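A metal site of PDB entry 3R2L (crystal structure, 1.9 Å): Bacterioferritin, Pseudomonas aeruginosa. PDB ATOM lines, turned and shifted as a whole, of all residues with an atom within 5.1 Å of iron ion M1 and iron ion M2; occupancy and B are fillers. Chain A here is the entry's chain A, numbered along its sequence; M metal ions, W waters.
OE2 of Glu 93 sits close to OH of Tyr 25 (2.5 Å).
OE1 of Gln 122 sits close to O of His 54 (3.1 Å).
Of the 9 residues printed, 3 come within 4 Å of iron ion M1.
The nearest printed residue that does not touch iron ion M1 is Thr 126 (4.2 Å).
Within 4 Å of iron ion M2: Glu 18, Glu 51 and His 54.
The nearest printed residue that does not touch iron ion M2 is Thr 126 (4.3 Å).
Water W1 is bound to iron ion M1 (2.0 Å).
Iron ion M1 is bound by OE2 of Glu 51, at 2.1 Å.
Iron ion M1 is bound by a ring nitrogen (ND1) of His 130 (2.1 Å).
OE2 of Glu 93 binds iron ion M1, at 2.2 Å.
The side-chain carboxylate (OE1) of Glu 93 binds iron ion M1, 2.4 Å away.
Iron ion M1 has five donor atoms within binding distance.
OE1 of Glu 18 is bound to iron ion M2 (2.0 Å).
Iron ion M2 is bound by water W1, at 2.1 Å.
OE1 of Glu 51 binds iron ion M2 (2.1 Å).
Iron ion M2 is bound by water W2.
ND1 of His 54 is bound to iron ion M2, 2.2 Å away.
Iron ion M2 has five donor atoms within binding distance.
Water W2 bridges the side-chain carboxylate (OE2) of Glu 18 (2.8 Å) and the side-chain amide nitrogen (NE2) of Gln 122 (3.3 Å).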
ATOM      1  N   GLU A  18     -11.858 -14.779 -17.973  1.00  0.00           N
ATOM      2  CA  GLU A  18     -11.662 -14.610 -19.440  1.00  0.00           C
ATOM      3  C   GLU A  18     -11.811 -15.965 -20.169  1.00  0.00           C
ATOM      4  O   GLU A  18     -12.402 -16.027 -21.264  1.00  0.00           O
ATOM      5  CB  GLU A  18     -10.275 -13.998 -19.768  1.00  0.00           C
ATOM      6  CG  GLU A  18     -10.114 -12.629 -19.166  1.00  0.00           C
ATOM      7  CD  GLU A  18     -11.165 -11.656 -19.675  1.00  0.00           C
ATOM      8  OE1 GLU A  18     -11.299 -11.527 -20.889  1.00  0.00           O
ATOM      9  OE2 GLU A  18     -11.874 -11.040 -18.877  1.00  0.00           O
ATOM     10  N   TYR A  25     -18.846 -17.251 -25.436  1.00  0.00           N
ATOM     11  CA  TYR A  25     -18.926 -16.818 -26.847  1.00  0.00           C
ATOM     12  C   TYR A  25     -18.772 -17.994 -27.816  1.00  0.00           C
ATOM     13  O   TYR A  25     -19.374 -17.985 -28.911  1.00  0.00           O
ATOM     14  CB  TYR A  25     -17.809 -15.822 -27.109  1.00  0.00           C
ATOM     15  CG  TYR A  25     -18.084 -14.457 -26.475  1.00  0.00           C
ATOM     16  CD1 TYR A  25     -19.353 -13.889 -26.542  1.00  0.00           C
ATOM     17  CD2 TYR A  25     -17.084 -13.727 -25.870  1.00  0.00           C
ATOM     18  CE1 TYR A  25     -19.616 -12.590 -26.035  1.00  0.00           C
ATOM     19  CE2 TYR A  25     -17.333 -12.457 -25.336  1.00  0.00           C
ATOM     20  CZ  TYR A  25     -18.613 -11.887 -25.423  1.00  0.00           C
ATOM     21  OH  TYR A  25     -18.895 -10.633 -24.908  1.00  0.00           O
ATOM     22  N   GLU A  51     -11.347 -12.828 -26.533  1.00  0.00           N
ATOM     23  CA  GLU A  51     -11.213 -13.262 -25.126  1.00  0.00           C
ATOM     24  C   GLU A  51     -10.056 -14.234 -24.972  1.00  0.00           C
ATOM     25  O   GLU A  51      -9.445 -14.303 -23.947  1.00  0.00           O
ATOM     26  CB  GLU A  51     -12.491 -13.949 -24.592  1.00  0.00           C
ATOM     27  CG  GLU A  51     -13.772 -13.127 -24.724  1.00  0.00           C
ATOM     28  CD  GLU A  51     -13.782 -11.808 -23.909  1.00  0.00           C
ATOM     29  OE1 GLU A  51     -12.794 -11.442 -23.284  1.00  0.00           O
ATOM     30  OE2 GLU A  51     -14.811 -11.155 -23.907  1.00  0.00           O
ATOM     31  N   HIS A  54      -7.234 -12.097 -24.517  1.00  0.00           N
ATOM     32  CA  HIS A  54      -7.228 -11.471 -23.180  1.00  0.00           C
ATOM     33  C   HIS A  54      -6.731 -12.487 -22.157  1.00  0.00           C
ATOM     34  O   HIS A  54      -5.907 -12.190 -21.308  1.00  0.00           O
ATOM     35  CB  HIS A  54      -8.627 -11.030 -22.766  1.00  0.00           C
ATOM     36  CG  HIS A  54      -9.103  -9.798 -23.452  1.00  0.00           C
ATOM     37  ND1 HIS A  54     -10.363  -9.292 -23.265  1.00  0.00           N
ATOM     38  CD2 HIS A  54      -8.486  -8.953 -24.315  1.00  0.00           C
ATOM     39  CE1 HIS A  54     -10.521  -8.205 -23.992  1.00  0.00           C
ATOM     40  NE2 HIS A  54      -9.390  -7.966 -24.633  1.00  0.00           N
ATOM     41  N   GLU A  93     -20.030  -9.371 -19.404  1.00  0.00           N
ATOM     42  CA  GLU A  93     -19.087  -8.267 -19.674  1.00  0.00           C
ATOM     43  C   GLU A  93     -19.151  -7.213 -18.557  1.00  0.00           C
ATOM     44  O   GLU A  93     -18.139  -6.636 -18.227  1.00  0.00           O
ATOM     45  CB  GLU A  93     -19.426  -7.581 -21.019  1.00  0.00           C
ATOM     46  CG  GLU A  93     -19.173  -8.501 -22.228  1.00  0.00           C
ATOM     47  CD  GLU A  93     -17.659  -8.727 -22.512  1.00  0.00           C
ATOM     48  OE1 GLU A  93     -16.794  -7.957 -22.031  1.00  0.00           O
ATOM     49  OE2 GLU A  93     -17.340  -9.671 -23.276  1.00  0.00           O
ATOM     50  N   VAL A  96     -17.094  -8.569 -15.807  1.00  0.00           N
ATOM     51  CA  VAL A  96     -15.672  -8.427 -16.157  1.00  0.00           C
ATOM     52  C   VAL A  96     -15.206  -6.983 -15.981  1.00  0.00           C
ATOM     53  O   VAL A  96     -14.113  -6.745 -15.456  1.00  0.00           O
ATOM     54  CB  VAL A  96     -15.395  -8.893 -17.619  1.00  0.00           C
ATOM     55  CG1 VAL A  96     -13.965  -8.498 -18.018  1.00  0.00           C
ATOM     56  CG2 VAL A  96     -15.585 -10.401 -17.722  1.00  0.00           C
ATOM     57  N   GLN A 122      -7.552  -4.217 -21.484  1.00  0.00           N
ATOM     58  CA  GLN A 122      -8.695  -5.100 -21.526  1.00  0.00           C
ATOM     59  C   GLN A 122      -9.963  -4.412 -21.101  1.00  0.00           C
ATOM     60  O   GLN A 122     -11.030  -4.718 -21.619  1.00  0.00           O
ATOM     61  CB  GLN A 122      -8.416  -6.335 -20.659  1.00  0.00           C
ATOM     62  CG  GLN A 122      -7.331  -7.175 -21.281  1.00  0.00           C
ATOM     63  CD  GLN A 122      -7.123  -8.511 -20.611  1.00  0.00           C
ATOM     64  OE1 GLN A 122      -6.083  -9.163 -20.827  1.00  0.00           O
ATOM     65  NE2 GLN A 122      -8.086  -8.937 -19.802  1.00  0.00           N
ATOM     66  N   THR A 126     -13.435  -4.183 -23.124  1.00  0.00           N
ATOM     67  CA  THR A 126     -14.699  -4.597 -22.500  1.00  0.00           C
ATOM     68  C   THR A 126     -15.784  -3.508 -22.603  1.00  0.00           C
ATOM     69  O   THR A 126     -16.914  -3.754 -23.049  1.00  0.00           O
ATOM     70  CB  THR A 126     -14.442  -4.931 -20.989  1.00  0.00           C
ATOM     71  OG1 THR A 126     -13.527  -6.045 -20.929  1.00  0.00           O
ATOM     72  CG2 THR A 126     -15.754  -5.236 -20.282  1.00  0.00           C
ATOM     73  N   HIS A 130     -16.854  -4.784 -26.545  1.00  0.00           N
ATOM     74  CA  HIS A 130     -17.747  -5.915 -26.201  1.00  0.00           C
ATOM     75  C   HIS A 130     -19.096  -5.463 -25.586  1.00  0.00           C
ATOM     76  O   HIS A 130     -20.157  -5.732 -26.135  1.00  0.00           O
ATOM     77  CB  HIS A 130     -17.027  -6.897 -25.249  1.00  0.00           C
ATOM     78  CG  HIS A 130     -15.721  -7.397 -25.794  1.00  0.00           C
ATOM     79  ND1 HIS A 130     -14.923  -8.304 -25.122  1.00  0.00           N
ATOM     80  CD2 HIS A 130     -15.083  -7.129 -26.962  1.00  0.00           C
ATOM     81  CE1 HIS A 130     -13.853  -8.565 -25.857  1.00  0.00           C
ATOM     82  NE2 HIS A 130     -13.921  -7.861 -26.969  1.00  0.00           N
HETATM   83 FE    FE M   1     -15.168  -9.222 -23.214  1.00  0.00          FE
HETATM   84 FE    FE M   2     -12.043  -9.989 -21.951  1.00  0.00          FE
HETATM   85  O   HOH W   1     -13.523  -8.570 -22.180  1.00  0.00           O
HETATM   86  O   HOH W   2     -11.336  -8.732 -20.318  1.00  0.00           O
